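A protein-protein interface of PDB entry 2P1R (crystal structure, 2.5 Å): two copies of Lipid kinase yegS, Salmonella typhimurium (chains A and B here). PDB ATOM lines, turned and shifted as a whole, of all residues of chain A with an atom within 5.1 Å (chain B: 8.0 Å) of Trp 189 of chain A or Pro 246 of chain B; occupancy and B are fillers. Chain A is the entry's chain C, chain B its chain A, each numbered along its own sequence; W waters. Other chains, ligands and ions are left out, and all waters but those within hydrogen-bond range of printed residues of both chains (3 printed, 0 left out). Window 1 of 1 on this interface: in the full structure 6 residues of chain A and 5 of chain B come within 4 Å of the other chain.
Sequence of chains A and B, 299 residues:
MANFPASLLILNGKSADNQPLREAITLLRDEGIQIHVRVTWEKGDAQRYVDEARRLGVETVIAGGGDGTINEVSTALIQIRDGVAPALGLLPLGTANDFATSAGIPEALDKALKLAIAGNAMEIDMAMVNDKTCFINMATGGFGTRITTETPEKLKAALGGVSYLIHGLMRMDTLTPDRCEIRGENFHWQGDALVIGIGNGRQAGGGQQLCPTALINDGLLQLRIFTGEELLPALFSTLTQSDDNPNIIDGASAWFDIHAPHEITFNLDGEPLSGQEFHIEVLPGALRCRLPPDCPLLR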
ATOM      1  N   CYS A 180      13.786  -1.080  -5.627  1.00  0.00           N
ATOM      2  CA  CYS A 180      14.312  -0.544  -6.871  1.00  0.00           C
ATOM      3  C   CYS A 180      13.545  -1.148  -8.045  1.00  0.00           C
ATOM      4  O   CYS A 180      13.059  -2.276  -7.958  1.00  0.00           O
ATOM      5  CB  CYS A 180      15.798  -0.861  -7.000  1.00  0.00           C
ATOM      6  SG  CYS A 180      16.117  -2.586  -7.315  1.00  0.00           S
ATOM      7  N   GLU A 181      13.430  -0.390  -9.134  1.00  0.00           N
ATOM      8  CA  GLU A 181      12.716  -0.846 -10.329  1.00  0.00           C
ATOM      9  C   GLU A 181      13.719  -1.114 -11.446  1.00  0.00           C
ATOM     10  O   GLU A 181      14.685  -0.369 -11.607  1.00  0.00           O
ATOM     11  CB  GLU A 181      11.717   0.221 -10.767  1.00  0.00           C
ATOM     12  CG  GLU A 181      10.791   0.669  -9.656  1.00  0.00           C
ATOM     13  CD  GLU A 181       9.939   1.856 -10.053  1.00  0.00           C
ATOM     14  OE1 GLU A 181       9.203   1.749 -11.059  1.00  0.00           O
ATOM     15  OE2 GLU A 181      10.004   2.894  -9.356  1.00  0.00           O
ATOM     16  N   ILE A 182      13.488  -2.165 -12.225  1.00  0.00           N
ATOM     17  CA  ILE A 182      14.411  -2.515 -13.297  1.00  0.00           C
ATOM     18  C   ILE A 182      13.722  -2.821 -14.620  1.00  0.00           C
ATOM     19  O   ILE A 182      12.863  -3.702 -14.682  1.00  0.00           O
ATOM     20  CB  ILE A 182      15.247  -3.759 -12.906  1.00  0.00           C
ATOM     21  CG1 ILE A 182      15.983  -3.510 -11.590  1.00  0.00           C
ATOM     22  CG2 ILE A 182      16.228  -4.104 -14.007  1.00  0.00           C
ATOM     23  CD1 ILE A 182      16.815  -4.692 -11.136  1.00  0.00           C
ATOM     24  N   PHE A 187      11.654  -7.131 -20.196  1.00  0.00           N
ATOM     25  CA  PHE A 187      12.011  -7.278 -18.800  1.00  0.00           C
ATOM     26  C   PHE A 187      11.516  -6.104 -17.971  1.00  0.00           C
ATOM     27  O   PHE A 187      11.816  -4.947 -18.266  1.00  0.00           O
ATOM     28  CB  PHE A 187      13.540  -7.411 -18.661  1.00  0.00           C
ATOM     29  CG  PHE A 187      14.001  -7.857 -17.290  1.00  0.00           C
ATOM     30  CD1 PHE A 187      14.129  -6.944 -16.245  1.00  0.00           C
ATOM     31  CD2 PHE A 187      14.281  -9.203 -17.040  1.00  0.00           C
ATOM     32  CE1 PHE A 187      14.531  -7.368 -14.962  1.00  0.00           C
ATOM     33  CE2 PHE A 187      14.681  -9.636 -15.769  1.00  0.00           C
ATOM     34  CZ  PHE A 187      14.804  -8.713 -14.731  1.00  0.00           C
ATOM     35  N   HIS A 188      10.748  -6.416 -16.935  1.00  0.00           N
ATOM     36  CA  HIS A 188      10.227  -5.407 -16.032  1.00  0.00           C
ATOM     37  C   HIS A 188      10.055  -6.045 -14.658  1.00  0.00           C
ATOM     38  O   HIS A 188       9.207  -6.910 -14.467  1.00  0.00           O
ATOM     39  CB  HIS A 188       8.890  -4.866 -16.538  1.00  0.00           C
ATOM     40  CG  HIS A 188       8.264  -3.873 -15.610  1.00  0.00           C
ATOM     41  ND1 HIS A 188       8.944  -2.772 -15.136  1.00  0.00           N
ATOM     42  CD2 HIS A 188       7.036  -3.832 -15.042  1.00  0.00           C
ATOM     43  CE1 HIS A 188       8.161  -2.096 -14.311  1.00  0.00           C
ATOM     44  NE2 HIS A 188       6.998  -2.718 -14.237  1.00  0.00           N
ATOM     45  N   TRP A 189      10.875  -5.632 -13.702  1.00  0.00           N
ATOM     46  CA  TRP A 189      10.791  -6.190 -12.361  1.00  0.00           C
ATOM     47  C   TRP A 189      10.872  -5.087 -11.330  1.00  0.00           C
ATOM     48  O   TRP A 189      11.471  -4.039 -11.566  1.00  0.00           O
ATOM     49  CB  TRP A 189      11.913  -7.200 -12.124  1.00  0.00           C
ATOM     50  CG  TRP A 189      11.911  -7.775 -10.744  1.00  0.00           C
ATOM     51  CD1 TRP A 189      11.263  -8.898 -10.319  1.00  0.00           C
ATOM     52  CD2 TRP A 189      12.605  -7.257  -9.608  1.00  0.00           C
ATOM     53  NE1 TRP A 189      11.517  -9.117  -8.988  1.00  0.00           N
ATOM     54  CE2 TRP A 189      12.339  -8.124  -8.526  1.00  0.00           C
ATOM     55  CE3 TRP A 189      13.428  -6.142  -9.397  1.00  0.00           C
ATOM     56  CZ2 TRP A 189      12.869  -7.912  -7.251  1.00  0.00           C
ATOM     57  CZ3 TRP A 189      13.951  -5.931  -8.128  1.00  0.00           C
ATOM     58  CH2 TRP A 189      13.669  -6.815  -7.070  1.00  0.00           C
ATOM     59  N   GLN A 190      10.277  -5.344 -10.174  1.00  0.00           N
ATOM     60  CA  GLN A 190      10.238  -4.371  -9.099  1.00  0.00           C
ATOM     61  C   GLN A 190      10.182  -5.085  -7.749  1.00  0.00           C
ATOM     62  O   GLN A 190       9.579  -6.152  -7.624  1.00  0.00           O
ATOM     63  CB  GLN A 190       9.012  -3.491  -9.315  1.00  0.00           C
ATOM     64  CG  GLN A 190       8.709  -2.471  -8.251  1.00  0.00           C
ATOM     65  CD  GLN A 190       7.483  -1.650  -8.611  1.00  0.00           C
ATOM     66  OE1 GLN A 190       6.953  -0.910  -7.784  1.00  0.00           O
ATOM     67  NE2 GLN A 190       7.027  -1.778  -9.858  1.00  0.00           N
ATOM     68  N   GLY A 191      10.830  -4.503  -6.747  1.00  0.00           N
ATOM     69  CA  GLY A 191      10.846  -5.107  -5.427  1.00  0.00           C
ATOM     70  C   GLY A 191      12.096  -4.766  -4.636  1.00  0.00           C
ATOM     71  O   GLY A 191      12.865  -3.876  -5.018  1.00  0.00           O
ATOM     72  N   ASP A 192      12.302  -5.462  -3.522  1.00  0.00           N
ATOM     73  CA  ASP A 192      13.477  -5.215  -2.700  1.00  0.00           C
ATOM     74  C   ASP A 192      14.616  -6.095  -3.178  1.00  0.00           C
ATOM     75  O   ASP A 192      14.467  -7.307  -3.301  1.00  0.00           O
ATOM     76  CB  ASP A 192      13.179  -5.496  -1.230  1.00  0.00           C
ATOM     77  CG  ASP A 192      12.102  -4.595  -0.678  1.00  0.00           C
ATOM     78  OD1 ASP A 192      12.090  -3.400  -1.038  1.00  0.00           O
ATOM     79  OD2 ASP A 192      11.274  -5.076   0.122  1.00  0.00           O
ATOM     80  N   ALA A 193      15.753  -5.472  -3.455  1.00  0.00           N
ATOM     81  CA  ALA A 193      16.913  -6.192  -3.951  1.00  0.00           C
ATOM     82  C   ALA A 193      18.078  -6.003  -3.012  1.00  0.00           C
ATOM     83  O   ALA A 193      18.233  -4.944  -2.409  1.00  0.00           O
ATOM     84  CB  ALA A 193      17.280  -5.687  -5.344  1.00  0.00           C
ATOM     85  N   ILE A 225      19.736 -10.552 -10.239  1.00  0.00           N
ATOM     86  CA  ILE A 225      19.230  -9.885  -9.049  1.00  0.00           C
ATOM     87  C   ILE A 225      19.204 -10.862  -7.890  1.00  0.00           C
ATOM     88  O   ILE A 225      18.691 -11.975  -8.025  1.00  0.00           O
ATOM     89  CB  ILE A 225      17.797  -9.353  -9.242  1.00  0.00           C
ATOM     90  CG1 ILE A 225      17.698  -8.551 -10.540  1.00  0.00           C
ATOM     91  CG2 ILE A 225      17.407  -8.477  -8.048  1.00  0.00           C
ATOM     92  CD1 ILE A 225      16.313  -7.979 -10.798  1.00  0.00           C
ATOM     93  N   THR A 227      17.750 -11.361  -4.259  1.00  0.00           N
ATOM     94  CA  THR A 227      16.758 -10.861  -3.317  1.00  0.00           C
ATOM     95  C   THR A 227      16.964 -11.570  -1.995  1.00  0.00           C
ATOM     96  O   THR A 227      17.789 -12.479  -1.895  1.00  0.00           O
ATOM     97  CB  THR A 227      15.321 -11.112  -3.817  1.00  0.00           C
ATOM     98  OG1 THR A 227      15.158 -12.495  -4.145  1.00  0.00           O
ATOM     99  CG2 THR A 227      15.034 -10.267  -5.048  1.00  0.00           C
ATOM    100  N   ILE A 249      17.121 -13.844  -9.627  1.00  0.00           N
ATOM    101  CA  ILE A 249      16.407 -13.606 -10.869  1.00  0.00           C
ATOM    102  C   ILE A 249      17.366 -13.173 -11.980  1.00  0.00           C
ATOM    103  O   ILE A 249      18.019 -12.126 -11.884  1.00  0.00           O
ATOM    104  CB  ILE A 249      15.321 -12.528 -10.686  1.00  0.00           C
ATOM    105  CG1 ILE A 249      14.352 -12.956  -9.576  1.00  0.00           C
ATOM    106  CG2 ILE A 249      14.574 -12.317 -12.001  1.00  0.00           C
ATOM    107  CD1 ILE A 249      13.300 -11.913  -9.226  1.00  0.00           C
ATOM    108  N   TRP B 189      10.996 -17.528   0.302  1.00  0.00           N
ATOM    109  CA  TRP B 189      10.786 -16.266  -0.411  1.00  0.00           C
ATOM    110  C   TRP B 189       9.844 -15.355   0.360  1.00  0.00           C
ATOM    111  O   TRP B 189       8.935 -15.819   1.049  1.00  0.00           O
ATOM    112  CB  TRP B 189      10.177 -16.537  -1.791  1.00  0.00           C
ATOM    113  CG  TRP B 189       9.913 -15.299  -2.607  1.00  0.00           C
ATOM    114  CD1 TRP B 189      10.785 -14.677  -3.455  1.00  0.00           C
ATOM    115  CD2 TRP B 189       8.716 -14.510  -2.613  1.00  0.00           C
ATOM    116  NE1 TRP B 189      10.207 -13.551  -3.984  1.00  0.00           N
ATOM    117  CE2 TRP B 189       8.937 -13.424  -3.485  1.00  0.00           C
ATOM    118  CE3 TRP B 189       7.477 -14.614  -1.966  1.00  0.00           C
ATOM    119  CZ2 TRP B 189       7.966 -12.443  -3.726  1.00  0.00           C
ATOM    120  CZ3 TRP B 189       6.508 -13.638  -2.207  1.00  0.00           C
ATOM    121  CH2 TRP B 189       6.762 -12.568  -3.079  1.00  0.00           C
ATOM    122  N   ASP B 192       6.048  -8.891  -2.179  1.00  0.00           N
ATOM    123  CA  ASP B 192       4.683  -8.633  -2.624  1.00  0.00           C
ATOM    124  C   ASP B 192       4.302  -9.632  -3.698  1.00  0.00           C
ATOM    125  O   ASP B 192       5.028  -9.812  -4.676  1.00  0.00           O
ATOM    126  CB  ASP B 192       4.533  -7.206  -3.145  1.00  0.00           C
ATOM    127  CG  ASP B 192       4.525  -6.180  -2.025  1.00  0.00           C
ATOM    128  OD1 ASP B 192       4.012  -6.503  -0.938  1.00  0.00           O
ATOM    129  OD2 ASP B 192       5.016  -5.049  -2.225  1.00  0.00           O
ATOM    130  N   ILE B 225       4.554 -18.594  -8.055  1.00  0.00           N
ATOM    131  CA  ILE B 225       4.216 -17.302  -7.490  1.00  0.00           C
ATOM    132  C   ILE B 225       4.230 -16.302  -8.635  1.00  0.00           C
ATOM    133  O   ILE B 225       5.195 -16.229  -9.390  1.00  0.00           O
ATOM    134  CB  ILE B 225       5.245 -16.830  -6.443  1.00  0.00           C
ATOM    135  CG1 ILE B 225       5.365 -17.847  -5.310  1.00  0.00           C
ATOM    136  CG2 ILE B 225       4.831 -15.472  -5.884  1.00  0.00           C
ATOM    137  CD1 ILE B 225       6.281 -17.389  -4.190  1.00  0.00           C
ATOM    138  N   PHE B 226       3.143 -15.557  -8.787  1.00  0.00           N
ATOM    139  CA  PHE B 226       3.083 -14.550  -9.824  1.00  0.00           C
ATOM    140  C   PHE B 226       3.244 -13.237  -9.088  1.00  0.00           C
ATOM    141  O   PHE B 226       2.478 -12.945  -8.166  1.00  0.00           O
ATOM    142  CB  PHE B 226       1.733 -14.575 -10.559  1.00  0.00           C
ATOM    143  CG  PHE B 226       1.462 -15.856 -11.310  1.00  0.00           C
ATOM    144  CD1 PHE B 226       0.865 -16.936 -10.681  1.00  0.00           C
ATOM    145  CD2 PHE B 226       1.839 -15.991 -12.639  1.00  0.00           C
ATOM    146  CE1 PHE B 226       0.646 -18.131 -11.364  1.00  0.00           C
ATOM    147  CE2 PHE B 226       1.626 -17.179 -13.327  1.00  0.00           C
ATOM    148  CZ  PHE B 226       1.029 -18.249 -12.687  1.00  0.00           C
ATOM    149  N   THR B 227       4.267 -12.472  -9.461  1.00  0.00           N
ATOM    150  CA  THR B 227       4.512 -11.164  -8.860  1.00  0.00           C
ATOM    151  C   THR B 227       4.214 -10.117  -9.924  1.00  0.00           C
ATOM    152  O   THR B 227       4.015 -10.445 -11.097  1.00  0.00           O
ATOM    153  CB  THR B 227       5.970 -11.015  -8.382  1.00  0.00           C
ATOM    154  OG1 THR B 227       6.866 -11.253  -9.482  1.00  0.00           O
ATOM    155  CG2 THR B 227       6.259 -12.007  -7.249  1.00  0.00           C
ATOM    156  N   GLY B 228       4.175  -8.855  -9.536  1.00  0.00           N
ATOM    157  CA  GLY B 228       3.871  -7.845 -10.529  1.00  0.00           C
ATOM    158  C   GLY B 228       2.424  -7.405 -10.426  1.00  0.00           C
ATOM    159  O   GLY B 228       1.638  -7.981  -9.673  1.00  0.00           O
ATOM    160  N   GLN B 241       9.056 -18.566 -21.979  1.00  0.00           N
ATOM    161  CA  GLN B 241       8.837 -17.185 -21.559  1.00  0.00           C
ATOM    162  C   GLN B 241       8.554 -17.176 -20.056  1.00  0.00           C
ATOM    163  O   GLN B 241       8.792 -16.179 -19.372  1.00  0.00           O
ATOM    164  CB  GLN B 241       7.647 -16.574 -22.306  1.00  0.00           C
ATOM    165  CG  GLN B 241       7.772 -16.570 -23.822  1.00  0.00           C
ATOM    166  CD  GLN B 241       6.571 -15.931 -24.499  1.00  0.00           C
ATOM    167  OE1 GLN B 241       5.434 -16.366 -24.315  1.00  0.00           O
ATOM    168  NE2 GLN B 241       6.819 -14.891 -25.289  1.00  0.00           N
ATOM    169  N   SER B 242       8.046 -18.300 -19.554  1.00  0.00           N
ATOM    170  CA  SER B 242       7.736 -18.439 -18.137  1.00  0.00           C
ATOM    171  C   SER B 242       9.021 -18.540 -17.314  1.00  0.00           C
ATOM    172  O   SER B 242       9.175 -17.841 -16.315  1.00  0.00           O
ATOM    173  CB  SER B 242       6.877 -19.679 -17.904  1.00  0.00           C
ATOM    174  OG  SER B 242       7.609 -20.850 -18.211  1.00  0.00           O
ATOM    175  N   ASP B 243       9.941 -19.408 -17.732  1.00  0.00           N
ATOM    176  CA  ASP B 243      11.208 -19.571 -17.019  1.00  0.00           C
ATOM    177  C   ASP B 243      12.036 -18.290 -17.055  1.00  0.00           C
ATOM    178  O   ASP B 243      12.910 -18.079 -16.218  1.00  0.00           O
ATOM    179  CB  ASP B 243      12.041 -20.709 -17.624  1.00  0.00           C
ATOM    180  CG  ASP B 243      11.400 -22.073 -17.443  1.00  0.00           C
ATOM    181  OD1 ASP B 243      10.815 -22.322 -16.364  1.00  0.00           O
ATOM    182  OD2 ASP B 243      11.497 -22.904 -18.374  1.00  0.00           O
ATOM    183  N   ASP B 244      11.769 -17.435 -18.031  1.00  0.00           N
ATOM    184  CA  ASP B 244      12.522 -16.205 -18.142  1.00  0.00           C
ATOM    185  C   ASP B 244      11.786 -15.014 -17.563  1.00  0.00           C
ATOM    186  O   ASP B 244      12.363 -13.937 -17.411  1.00  0.00           O
ATOM    187  CB  ASP B 244      12.888 -15.946 -19.604  1.00  0.00           C
ATOM    188  CG  ASP B 244      13.901 -16.950 -20.136  1.00  0.00           C
ATOM    189  OD1 ASP B 244      14.977 -17.100 -19.515  1.00  0.00           O
ATOM    190  OD2 ASP B 244      13.627 -17.587 -21.175  1.00  0.00           O
ATOM    191  N   ASN B 245      10.513 -15.208 -17.228  1.00  0.00           N
ATOM    192  CA  ASN B 245       9.718 -14.126 -16.658  1.00  0.00           C
ATOM    193  C   ASN B 245      10.179 -13.845 -15.232  1.00  0.00           C
ATOM    194  O   ASN B 245      10.009 -14.657 -14.335  1.00  0.00           O
ATOM    195  CB  ASN B 245       8.232 -14.490 -16.645  1.00  0.00           C
ATOM    196  CG  ASN B 245       7.339 -13.292 -16.366  1.00  0.00           C
ATOM    197  OD1 ASN B 245       7.744 -12.324 -15.708  1.00  0.00           O
ATOM    198  ND2 ASN B 245       6.105 -13.357 -16.859  1.00  0.00           N
ATOM    199  N   PRO B 246      10.756 -12.674 -15.005  1.00  0.00           N
ATOM    200  CA  PRO B 246      11.230 -12.327 -13.666  1.00  0.00           C
ATOM    201  C   PRO B 246      10.120 -12.321 -12.606  1.00  0.00           C
ATOM    202  O   PRO B 246      10.381 -12.507 -11.413  1.00  0.00           O
ATOM    203  CB  PRO B 246      11.851 -10.950 -13.879  1.00  0.00           C
ATOM    204  CG  PRO B 246      10.985 -10.366 -14.989  1.00  0.00           C
ATOM    205  CD  PRO B 246      10.837 -11.527 -15.929  1.00  0.00           C
ATOM    206  N   ASN B 247       8.884 -12.114 -13.046  1.00  0.00           N
ATOM    207  CA  ASN B 247       7.747 -12.066 -12.134  1.00  0.00           C
ATOM    208  C   ASN B 247       7.061 -13.405 -11.887  1.00  0.00           C
ATOM    209  O   ASN B 247       5.988 -13.450 -11.279  1.00  0.00           O
ATOM    210  CB  ASN B 247       6.713 -11.059 -12.630  1.00  0.00           C
ATOM    211  CG  ASN B 247       7.184  -9.630 -12.499  1.00  0.00           C
ATOM    212  OD1 ASN B 247       7.442  -9.146 -11.399  1.00  0.00           O
ATOM    213  ND2 ASN B 247       7.295  -8.945 -13.626  1.00  0.00           N
ATOM    214  N   ILE B 248       7.667 -14.485 -12.375  1.00  0.00           N
ATOM    215  CA  ILE B 248       7.143 -15.827 -12.170  1.00  0.00           C
ATOM    216  C   ILE B 248       8.219 -16.596 -11.396  1.00  0.00           C
ATOM    217  O   ILE B 248       9.352 -16.693 -11.845  1.00  0.00           O
ATOM    218  CB  ILE B 248       6.852 -16.542 -13.511  1.00  0.00           C
ATOM    219  CG1 ILE B 248       5.653 -15.892 -14.204  1.00  0.00           C
ATOM    220  CG2 ILE B 248       6.575 -18.020 -13.282  1.00  0.00           C
ATOM    221  CD1 ILE B 248       5.323 -16.499 -15.573  1.00  0.00           C
ATOM    222  N   ILE B 249       7.869 -17.107 -10.218  1.00  0.00           N
ATOM    223  CA  ILE B 249       8.812 -17.852  -9.389  1.00  0.00           C
ATOM    224  C   ILE B 249       8.303 -19.258  -9.141  1.00  0.00           C
ATOM    225  O   ILE B 249       7.181 -19.452  -8.675  1.00  0.00           O
ATOM    226  CB  ILE B 249       9.030 -17.169  -8.030  1.00  0.00           C
ATOM    227  CG1 ILE B 249       9.566 -15.751  -8.246  1.00  0.00           C
ATOM    228  CG2 ILE B 249      10.001 -17.980  -7.198  1.00  0.00           C
ATOM    229  CD1 ILE B 249       9.770 -14.946  -6.978  1.00  0.00           C
HETATM  230  O   HOH W   1      12.980 -13.150  -5.716  1.00  0.00           O
HETATM  231  O   HOH W   2       7.551  -6.654 -10.535  1.00  0.00           O
HETATM  232  O   HOH W   3       9.702 -11.565  -8.822  1.00  0.00           O
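Water W2 lies within hydrogen-bond range of OD1 of Asn 247 of chain B (2.6 Å) and N of Gln 190 of chain A (3.0 Å). Water W1 lies within hydrogen-bond range of OG1 of Thr 227 of chain A (2.8 Å) and NE1 of Trp 189 of chain B (3.3 Å). Water W3 lies within hydrogen-bond range of the backbone carbonyl oxygen (O) of Pro 246 of chain B (2.8 Å), the side-chain hydroxyl (OG1) of Thr 227 of chain B (2.9 Å) and the indole nitrogen (NE1) of Trp 189 of chain A (3.1 Å).
Phe 187 of chain A touches Pro 246 of chain B (CE2 to CB, 3.6 Å). Pro 246 of chain B touches His 188 of chain A (CG to O, 3.9 Å). CD1 of Trp 189 of chain A touches O of Pro 246 of chain B, at 3.9 Å. Trp 189 of chain A touches Asn 247 of chain B. Pro 246 of chain B touches Ile 249 of chain A.
Trp 189 of chain A touches just these residues of chain B: Pro 246 and Asn 247. Of chain A, only Phe 187 (3.6 Å), His 188 (3.9 Å), Trp 189 (3.9 Å) and Ile 249 (3.6 Å) come within 4 Å of Pro 246 of chain B. No residue of chain B comes within 4 Å of Gly 191 of chain A. Of the printed residues of chain A, Asn 247 of chain B touches His 188 and Trp 189. Of the printed residues of chain B, His 188 of chain A touches Pro 246 (3.9 Å) and Asn 247 (2.9 Å). Of the printed residues of chain B, Phe 187 of chain A touches Pro 246 (3.6 Å). Printed residues of chain B within 4 Å of Ile 249 of chain A: Pro 246. The nearest printed residue of chain A that does not touch Pro 246 of chain B is Ile 225 of chain A (6.2 Å).
Of the 15 printed residues of chain B, 2 touch a printed residue of chain A. Hydrophobic or aromatic side chains of chain B within 4 Å of the printed part of chain A: Pro 246. Printed residues of chain A that touch a printed residue of chain B: Phe 187, His 188, Trp 189 and Ile 249. Hydrophobic or aromatic side chains of chain A within 4 Å of the printed part of chain B: Phe 187, Trp 189 and Ile 249.
ND2 of Asn 247 of chain B lies within hydrogen-bond range of O of His 188 of chain A, 2.9 Å away.
Positions printed for both chains: 189, 192, 225, 227 and 249. Of the 6 pairs that touch across the chains among the printed residues, none has its exchanged pair printed and touching as well.
The backbone NH (N) of Asn 247 of chain B sits at hydrogen-bond distance from the side-chain amide oxygen (OD1) of Asn 245 of chain B (2.9 Å). The backbone NH of Thr 227 of chain B sits at hydrogen-bond distance from the backbone carbonyl oxygen of Asn 247 of chain B, 2.7 Å away. The backbone NH (N) of Ile 182 of chain A sits at hydrogen-bond distance from the backbone carbonyl oxygen (O) of Trp 189 of chain A, 2.8 Å away. N of Ile 225 of chain A lies within hydrogen-bond range of O of Ile 249 of chain A, 2.9 Å away.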
